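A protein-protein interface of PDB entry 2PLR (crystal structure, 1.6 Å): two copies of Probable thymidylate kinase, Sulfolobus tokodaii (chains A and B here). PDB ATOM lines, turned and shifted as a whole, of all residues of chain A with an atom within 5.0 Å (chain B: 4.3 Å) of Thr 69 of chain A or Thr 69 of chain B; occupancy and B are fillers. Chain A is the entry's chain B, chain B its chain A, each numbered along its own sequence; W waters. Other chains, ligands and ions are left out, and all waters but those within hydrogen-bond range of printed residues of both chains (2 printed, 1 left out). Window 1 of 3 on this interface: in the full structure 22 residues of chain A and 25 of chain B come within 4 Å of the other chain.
OG1 of Thr 62 of chain B sits at hydrogen-bond distance from OG of Ser 72 of chain A (2.9 Å). The side-chain hydroxyl (OG1) of Thr 69 of chain A lies close to the backbone carbonyl oxygen (O) of Leu 65 of chain B. The backbone carbonyl oxygen (O) of Leu 65 of chain A lies close to the side-chain hydroxyl (OG1) of Thr 69 of chain B. OG1 of Thr 69 of chain B is in hydrogen-bond range of OG1 of Thr 69 of chain A, at 3.1 Å. OG1 of Thr 62 of chain A lies within hydrogen-bond range of OG of Ser 72 of chain B (2.7 Å).
N of Ile 45 of chain B lies within hydrogen-bond range of OD1 of Asp 70 of chain B, at 3.4 Å. OG1 of Thr 69 of chain B is in hydrogen-bond range of O of Leu 65 of chain B (2.6 Å). O of Thr 69 of chain B is in hydrogen-bond range of OG of Ser 72 of chain B, at 2.7 Å. The backbone carbonyl oxygen (O) of Leu 65 of chain A lies within hydrogen-bond range of the side-chain hydroxyl (OG1) of Thr 69 of chain A (2.7 Å). The side-chain hydroxyl (OG) of Ser 72 of chain A lies within hydrogen-bond range of the backbone carbonyl oxygen (O) of Thr 69 of chain A.
Ile 45 of chain B touches Thr 62 of chain A. CG2 of Thr 69 of chain B touches CG2 of Thr 62 of chain A (3.998 Å). Thr 62 of chain A touches Asp 73 of chain B. Leu 65 of chain A touches Ala 68 of chain B (CD1 to O, 3.8 Å). Ser 72 of chain B touches Leu 65 of chain A (CB to CD1, 3.7 Å). CG2 of Thr 69 of chain B touches CG1 of Ile 66 of chain A, 3.6 Å away. O of Ala 68 of chain A touches CD1 of Leu 65 of chain B (3.7 Å). Thr 69 of chain A touches Ile 66 of chain B (CG2 to CG1, 3.6 Å). Leu 65 of chain B touches Ser 72 of chain A (CD1 to CB, 3.5 Å). Asp 73 of chain A touches Thr 62 of chain B (N to OG1, 3.5 Å).
Of chain B, only Leu 65, Ile 66 and Thr 69 come within 4 Å of Thr 69 of chain A. Printed residues of chain A within 4 Å of Thr 69 of chain B: Thr 62 (3.998 Å), Leu 65 (3.2 Å), Ile 66 (3.6 Å) and Thr 69 (3.1 Å). Of the printed residues of chain A, Ile 45 of chain B touches Thr 62. Of the printed residues of chain B, Ile 66 of chain A touches Thr 69 (3.6 Å). Printed residues of chain A within 4 Å of Leu 65 of chain B: Ala 68 (3.7 Å), Thr 69 (3.3 Å) and Ser 72 (3.5 Å). The nearest residue of chain B that does not touch Thr 69 of chain A is Thr 62 of chain B (4.1 Å). The nearest printed residue of chain A that does not touch Thr 69 of chain B is His 67 of chain A (6.2 Å).
Of the 11 printed residues of chain B, 8 touch a printed residue of chain A. Along chain B the printed residues that touch a printed residue of chain A span positions 45 to 73. Hydrophobic or aromatic side chains of chain A that line the printed part of chain B: Leu 65 and Ile 66. Among the printed residues, no Asp or Glu carboxylate lies within 4 Å of a Lys or Arg side-chain nitrogen of the other chain.
Thr 62 of chain A touches Thr 69 of chain B, but with the chains exchanged Thr 69 of chain A does not touch Thr 62 of chain B (4.1 Å). Thr 62 of chain A touches Asp 73 of chain B, and with the chains exchanged Asp 73 of chain A touches Thr 62 of chain B. Leu 65 of chain A touches Ala 68 of chain B, and with the chains exchanged Ala 68 of chain A touches Leu 65 of chain B. Leu 65 of chain A touches Thr 69 of chain B, and with the chains exchanged Thr 69 of chain A touches Leu 65 of chain B. Of the 15 pairs that touch across the chains among the printed residues, 13 have their exchanged pair printed and touching as well.
Water W1 bridges the side-chain hydroxyl (OG1) of Thr 62 of chain B (2.7 Å) and the side-chain carboxylate (OD1) of Asp 73 of chain A (2.8 Å). Water W2 bridges the side-chain hydroxyl (OG1) of Thr 62 of chain A and the side-chain carboxylate (OD2) of Asp 73 of chain B.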
ATOM      1  N   TRP A  44      11.465   1.088  15.861  1.00  0.00           N
ATOM      2  CA  TRP A  44      12.610   1.989  15.861  1.00  0.00           C
ATOM      3  C   TRP A  44      12.404   3.298  16.622  1.00  0.00           C
ATOM      4  O   TRP A  44      13.373   3.905  17.072  1.00  0.00           O
ATOM      5  CB  TRP A  44      13.077   2.281  14.429  1.00  0.00           C
ATOM      6  CG  TRP A  44      12.041   2.847  13.512  1.00  0.00           C
ATOM      7  CD1 TRP A  44      11.182   2.150  12.708  1.00  0.00           C
ATOM      8  CD2 TRP A  44      11.791   4.233  13.261  1.00  0.00           C
ATOM      9  NE1 TRP A  44      10.417   3.021  11.965  1.00  0.00           N
ATOM     10  CE2 TRP A  44      10.770   4.305  12.286  1.00  0.00           C
ATOM     11  CE3 TRP A  44      12.332   5.425  13.762  1.00  0.00           C
ATOM     12  CZ2 TRP A  44      10.280   5.524  11.803  1.00  0.00           C
ATOM     13  CZ3 TRP A  44      11.843   6.637  13.281  1.00  0.00           C
ATOM     14  CH2 TRP A  44      10.829   6.675  12.310  1.00  0.00           C
ATOM     15  N   THR A  62      13.195  17.420  17.888  1.00  0.00           N
ATOM     16  CA  THR A  62      13.625  16.142  17.348  1.00  0.00           C
ATOM     17  C   THR A  62      12.532  15.089  17.516  1.00  0.00           C
ATOM     18  O   THR A  62      12.321  14.255  16.641  1.00  0.00           O
ATOM     19  CB  THR A  62      14.909  15.669  18.033  1.00  0.00           C
ATOM     20  OG1 THR A  62      15.920  16.670  17.864  1.00  0.00           O
ATOM     21  CG2 THR A  62      15.391  14.355  17.416  1.00  0.00           C
ATOM     22  N   LEU A  65      10.064  15.585  14.823  1.00  0.00           N
ATOM     23  CA  LEU A  65      10.575  15.119  13.544  1.00  0.00           C
ATOM     24  C   LEU A  65      10.634  13.600  13.432  1.00  0.00           C
ATOM     25  O   LEU A  65      10.416  13.048  12.358  1.00  0.00           O
ATOM     26  CB  LEU A  65      11.947  15.746  13.279  1.00  0.00           C
ATOM     27  CG  LEU A  65      11.861  17.247  12.966  1.00  0.00           C
ATOM     28  CD1 LEU A  65      13.251  17.853  12.975  1.00  0.00           C
ATOM     29  CD2 LEU A  65      11.196  17.467  11.609  1.00  0.00           C
ATOM     30  N   ILE A  66      10.926  12.923  14.540  1.00  0.00           N
ATOM     31  CA  ILE A  66      10.978  11.465  14.529  1.00  0.00           C
ATOM     32  C   ILE A  66       9.612  10.917  14.133  1.00  0.00           C
ATOM     33  O   ILE A  66       9.504  10.023  13.293  1.00  0.00           O
ATOM     34  CB  ILE A  66      11.344  10.904  15.922  1.00  0.00           C
ATOM     35  CG1 ILE A  66      12.822  11.164  16.213  1.00  0.00           C
ATOM     36  CG2 ILE A  66      11.027   9.416  15.989  1.00  0.00           C
ATOM     37  CD1 ILE A  66      13.196  10.966  17.674  1.00  0.00           C
ATOM     38  N   HIS A  67       8.559  11.457  14.740  1.00  0.00           N
ATOM     39  CA  HIS A  67       7.219  10.987  14.421  1.00  0.00           C
ATOM     40  C   HIS A  67       6.769  11.385  13.021  1.00  0.00           C
ATOM     41  O   HIS A  67       6.066  10.627  12.358  1.00  0.00           O
ATOM     42  CB  HIS A  67       6.212  11.478  15.462  1.00  0.00           C
ATOM     43  CG  HIS A  67       6.163  10.629  16.693  1.00  0.00           C
ATOM     44  ND1 HIS A  67       6.878  10.919  17.833  1.00  0.00           N
ATOM     45  CD2 HIS A  67       5.505   9.470  16.945  1.00  0.00           C
ATOM     46  CE1 HIS A  67       6.664   9.979  18.737  1.00  0.00           C
ATOM     47  NE2 HIS A  67       5.835   9.088  18.223  1.00  0.00           N
ATOM     48  N   ALA A  68       7.178  12.565  12.562  1.00  0.00           N
ATOM     49  CA  ALA A  68       6.805  13.008  11.222  1.00  0.00           C
ATOM     50  C   ALA A  68       7.476  12.093  10.200  1.00  0.00           C
ATOM     51  O   ALA A  68       6.901  11.774   9.162  1.00  0.00           O
ATOM     52  CB  ALA A  68       7.235  14.462  11.000  1.00  0.00           C
ATOM     53  N   THR A  69       8.699  11.671  10.503  1.00  0.00           N
ATOM     54  CA  THR A  69       9.436  10.777   9.618  1.00  0.00           C
ATOM     55  C   THR A  69       8.682   9.459   9.494  1.00  0.00           C
ATOM     56  O   THR A  69       8.450   8.970   8.389  1.00  0.00           O
ATOM     57  CB  THR A  69      10.851  10.505  10.166  1.00  0.00           C
ATOM     58  OG1 THR A  69      11.568  11.741  10.252  1.00  0.00           O
ATOM     59  CG2 THR A  69      11.607   9.543   9.248  1.00  0.00           C
ATOM     60  N   ASP A  70       8.296   8.892  10.632  1.00  0.00           N
ATOM     61  CA  ASP A  70       7.547   7.640  10.638  1.00  0.00           C
ATOM     62  C   ASP A  70       6.228   7.808   9.884  1.00  0.00           C
ATOM     63  O   ASP A  70       5.859   6.974   9.055  1.00  0.00           O
ATOM     64  CB  ASP A  70       7.259   7.204  12.076  1.00  0.00           C
ATOM     65  CG  ASP A  70       6.430   5.941  12.142  1.00  0.00           C
ATOM     66  OD1 ASP A  70       6.874   4.915  11.593  1.00  0.00           O
ATOM     67  OD2 ASP A  70       5.333   5.979  12.737  1.00  0.00           O
ATOM     68  N   PHE A  71       5.515   8.897  10.163  1.00  0.00           N
ATOM     69  CA  PHE A  71       4.245   9.142   9.494  1.00  0.00           C
ATOM     70  C   PHE A  71       4.411   9.276   7.981  1.00  0.00           C
ATOM     71  O   PHE A  71       3.609   8.746   7.216  1.00  0.00           O
ATOM     72  CB  PHE A  71       3.572  10.403  10.060  1.00  0.00           C
ATOM     73  CG  PHE A  71       2.293  10.778   9.351  1.00  0.00           C
ATOM     74  CD1 PHE A  71       2.305  11.668   8.283  1.00  0.00           C
ATOM     75  CD2 PHE A  71       1.083  10.201   9.728  1.00  0.00           C
ATOM     76  CE1 PHE A  71       1.133  11.977   7.592  1.00  0.00           C
ATOM     77  CE2 PHE A  71      -0.095  10.502   9.043  1.00  0.00           C
ATOM     78  CZ  PHE A  71      -0.070  11.390   7.974  1.00  0.00           C
ATOM     79  N   SER A  72       5.459   9.975   7.545  1.00  0.00           N
ATOM     80  CA  SER A  72       5.672  10.156   6.115  1.00  0.00           C
ATOM     81  C   SER A  72       5.845   8.819   5.403  1.00  0.00           C
ATOM     82  O   SER A  72       5.371   8.638   4.284  1.00  0.00           O
ATOM     83  CB  SER A  72       6.897  11.046   5.849  1.00  0.00           C
ATOM     84  OG  SER A  72       8.117  10.354   6.062  1.00  0.00           O
ATOM     85  N   ASP A  73       6.518   7.882   6.059  1.00  0.00           N
ATOM     86  CA  ASP A  73       6.759   6.573   5.470  1.00  0.00           C
ATOM     87  C   ASP A  73       5.455   5.806   5.288  1.00  0.00           C
ATOM     88  O   ASP A  73       5.155   5.304   4.205  1.00  0.00           O
ATOM     89  CB  ASP A  73       7.718   5.777   6.355  1.00  0.00           C
ATOM     90  CG  ASP A  73       8.070   4.427   5.769  1.00  0.00           C
ATOM     91  OD1 ASP A  73       8.638   4.389   4.658  1.00  0.00           O
ATOM     92  OD2 ASP A  73       7.779   3.405   6.426  1.00  0.00           O
ATOM     93  N   ILE B  45      20.755   9.041  15.165  1.00  0.00           N
ATOM     94  CA  ILE B  45      19.360   8.863  14.763  1.00  0.00           C
ATOM     95  C   ILE B  45      19.309   8.407  13.310  1.00  0.00           C
ATOM     96  O   ILE B  45      18.566   7.489  12.957  1.00  0.00           O
ATOM     97  CB  ILE B  45      18.555  10.160  14.944  1.00  0.00           C
ATOM     98  CG1 ILE B  45      18.423  10.461  16.439  1.00  0.00           C
ATOM     99  CG2 ILE B  45      17.174  10.021  14.303  1.00  0.00           C
ATOM    100  CD1 ILE B  45      17.676  11.743  16.757  1.00  0.00           C
ATOM    101  N   THR B  62      10.684  10.869   2.897  1.00  0.00           N
ATOM    102  CA  THR B  62      11.100  10.232   4.142  1.00  0.00           C
ATOM    103  C   THR B  62      12.600  10.429   4.380  1.00  0.00           C
ATOM    104  O   THR B  62      13.028  10.659   5.516  1.00  0.00           O
ATOM    105  CB  THR B  62      10.728   8.735   4.144  1.00  0.00           C
ATOM    106  OG1 THR B  62       9.304   8.609   4.023  1.00  0.00           O
ATOM    107  CG2 THR B  62      11.169   8.071   5.445  1.00  0.00           C
ATOM    108  N   LEU B  65      13.142  13.828   5.718  1.00  0.00           N
ATOM    109  CA  LEU B  65      12.809  13.918   7.135  1.00  0.00           C
ATOM    110  C   LEU B  65      13.822  13.209   8.032  1.00  0.00           C
ATOM    111  O   LEU B  65      14.118  13.688   9.125  1.00  0.00           O
ATOM    112  CB  LEU B  65      11.393  13.383   7.368  1.00  0.00           C
ATOM    113  CG  LEU B  65      10.329  14.379   6.890  1.00  0.00           C
ATOM    114  CD1 LEU B  65       8.987  13.672   6.699  1.00  0.00           C
ATOM    115  CD2 LEU B  65      10.203  15.522   7.893  1.00  0.00           C
ATOM    116  N   ILE B  66      14.362  12.079   7.581  1.00  0.00           N
ATOM    117  CA  ILE B  66      15.364  11.372   8.377  1.00  0.00           C
ATOM    118  C   ILE B  66      16.560  12.294   8.570  1.00  0.00           C
ATOM    119  O   ILE B  66      17.077  12.443   9.678  1.00  0.00           O
ATOM    120  CB  ILE B  66      15.860  10.092   7.672  1.00  0.00           C
ATOM    121  CG1 ILE B  66      14.735   9.057   7.630  1.00  0.00           C
ATOM    122  CG2 ILE B  66      17.076   9.520   8.414  1.00  0.00           C
ATOM    123  CD1 ILE B  66      15.075   7.810   6.825  1.00  0.00           C
ATOM    124  N   HIS B  67      16.997  12.919   7.485  1.00  0.00           N
ATOM    125  CA  HIS B  67      18.144  13.814   7.563  1.00  0.00           C
ATOM    126  C   HIS B  67      17.859  15.034   8.436  1.00  0.00           C
ATOM    127  O   HIS B  67      18.706  15.437   9.230  1.00  0.00           O
ATOM    128  CB  HIS B  67      18.580  14.252   6.160  1.00  0.00           C
ATOM    129  CG  HIS B  67      18.931  13.111   5.254  1.00  0.00           C
ATOM    130  ND1 HIS B  67      19.272  11.860   5.720  1.00  0.00           N
ATOM    131  CD2 HIS B  67      19.012  13.045   3.902  1.00  0.00           C
ATOM    132  CE1 HIS B  67      19.546  11.072   4.696  1.00  0.00           C
ATOM    133  NE2 HIS B  67      19.396  11.762   3.584  1.00  0.00           N
ATOM    134  N   ALA B  68      16.669  15.618   8.310  1.00  0.00           N
ATOM    135  CA  ALA B  68      16.329  16.785   9.121  1.00  0.00           C
ATOM    136  C   ALA B  68      16.263  16.399  10.599  1.00  0.00           C
ATOM    137  O   ALA B  68      16.676  17.166  11.473  1.00  0.00           O
ATOM    138  CB  ALA B  68      14.990  17.370   8.672  1.00  0.00           C
ATOM    139  N   THR B  69      15.738  15.209  10.874  1.00  0.00           N
ATOM    140  CA  THR B  69      15.622  14.726  12.248  1.00  0.00           C
ATOM    141  C   THR B  69      17.016  14.574  12.841  1.00  0.00           C
ATOM    142  O   THR B  69      17.297  15.056  13.939  1.00  0.00           O
ATOM    143  CB  THR B  69      14.920  13.360  12.303  1.00  0.00           C
ATOM    144  OG1 THR B  69      13.623  13.469  11.707  1.00  0.00           O
ATOM    145  CG2 THR B  69      14.774  12.892  13.747  1.00  0.00           C
ATOM    146  N   ASP B  70      17.890  13.899  12.105  1.00  0.00           N
ATOM    147  CA  ASP B  70      19.250  13.692  12.575  1.00  0.00           C
ATOM    148  C   ASP B  70      19.936  15.036  12.784  1.00  0.00           C
ATOM    149  O   ASP B  70      20.617  15.246  13.791  1.00  0.00           O
ATOM    150  CB  ASP B  70      20.033  12.850  11.562  1.00  0.00           C
ATOM    151  CG  ASP B  70      21.386  12.407  12.092  1.00  0.00           C
ATOM    152  OD1 ASP B  70      21.422  11.617  13.059  1.00  0.00           O
ATOM    153  OD2 ASP B  70      22.411  12.849  11.538  1.00  0.00           O
ATOM    154  N   PHE B  71      19.760  15.957  11.841  1.00  0.00           N
ATOM    155  CA  PHE B  71      20.390  17.259  11.989  1.00  0.00           C
ATOM    156  C   PHE B  71      19.846  18.047  13.181  1.00  0.00           C
ATOM    157  O   PHE B  71      20.603  18.757  13.844  1.00  0.00           O
ATOM    158  CB  PHE B  71      20.238  18.110  10.731  1.00  0.00           C
ATOM    159  CG  PHE B  71      20.906  19.450  10.843  1.00  0.00           C
ATOM    160  CD1 PHE B  71      22.289  19.534  10.962  1.00  0.00           C
ATOM    161  CD2 PHE B  71      20.155  20.618  10.884  1.00  0.00           C
ATOM    162  CE1 PHE B  71      22.917  20.770  11.126  1.00  0.00           C
ATOM    163  CE2 PHE B  71      20.773  21.859  11.048  1.00  0.00           C
ATOM    164  CZ  PHE B  71      22.154  21.932  11.168  1.00  0.00           C
ATOM    165  N   SER B  72      18.546  17.935  13.456  1.00  0.00           N
ATOM    166  CA  SER B  72      17.975  18.674  14.581  1.00  0.00           C
ATOM    167  C   SER B  72      18.673  18.273  15.873  1.00  0.00           C
ATOM    168  O   SER B  72      18.851  19.101  16.769  1.00  0.00           O
ATOM    169  CB  SER B  72      16.458  18.439  14.698  1.00  0.00           C
ATOM    170  OG  SER B  72      16.144  17.145  15.179  1.00  0.00           O
ATOM    171  N   ASP B  73      19.078  17.008  15.967  1.00  0.00           N
ATOM    172  CA  ASP B  73      19.773  16.539  17.162  1.00  0.00           C
ATOM    173  C   ASP B  73      21.213  17.060  17.165  1.00  0.00           C
ATOM    174  O   ASP B  73      21.705  17.549  18.180  1.00  0.00           O
ATOM    175  CB  ASP B  73      19.769  15.010  17.231  1.00  0.00           C
ATOM    176  CG  ASP B  73      20.335  14.492  18.539  1.00  0.00           C
ATOM    177  OD1 ASP B  73      21.502  14.053  18.558  1.00  0.00           O
ATOM    178  OD2 ASP B  73      19.614  14.544  19.556  1.00  0.00           O
HETATM  179  O   HOH W   1       9.144   6.286   2.703  1.00  0.00           O
HETATM  180  O   HOH W   2      17.325  16.057  20.175  1.00  0.00           O
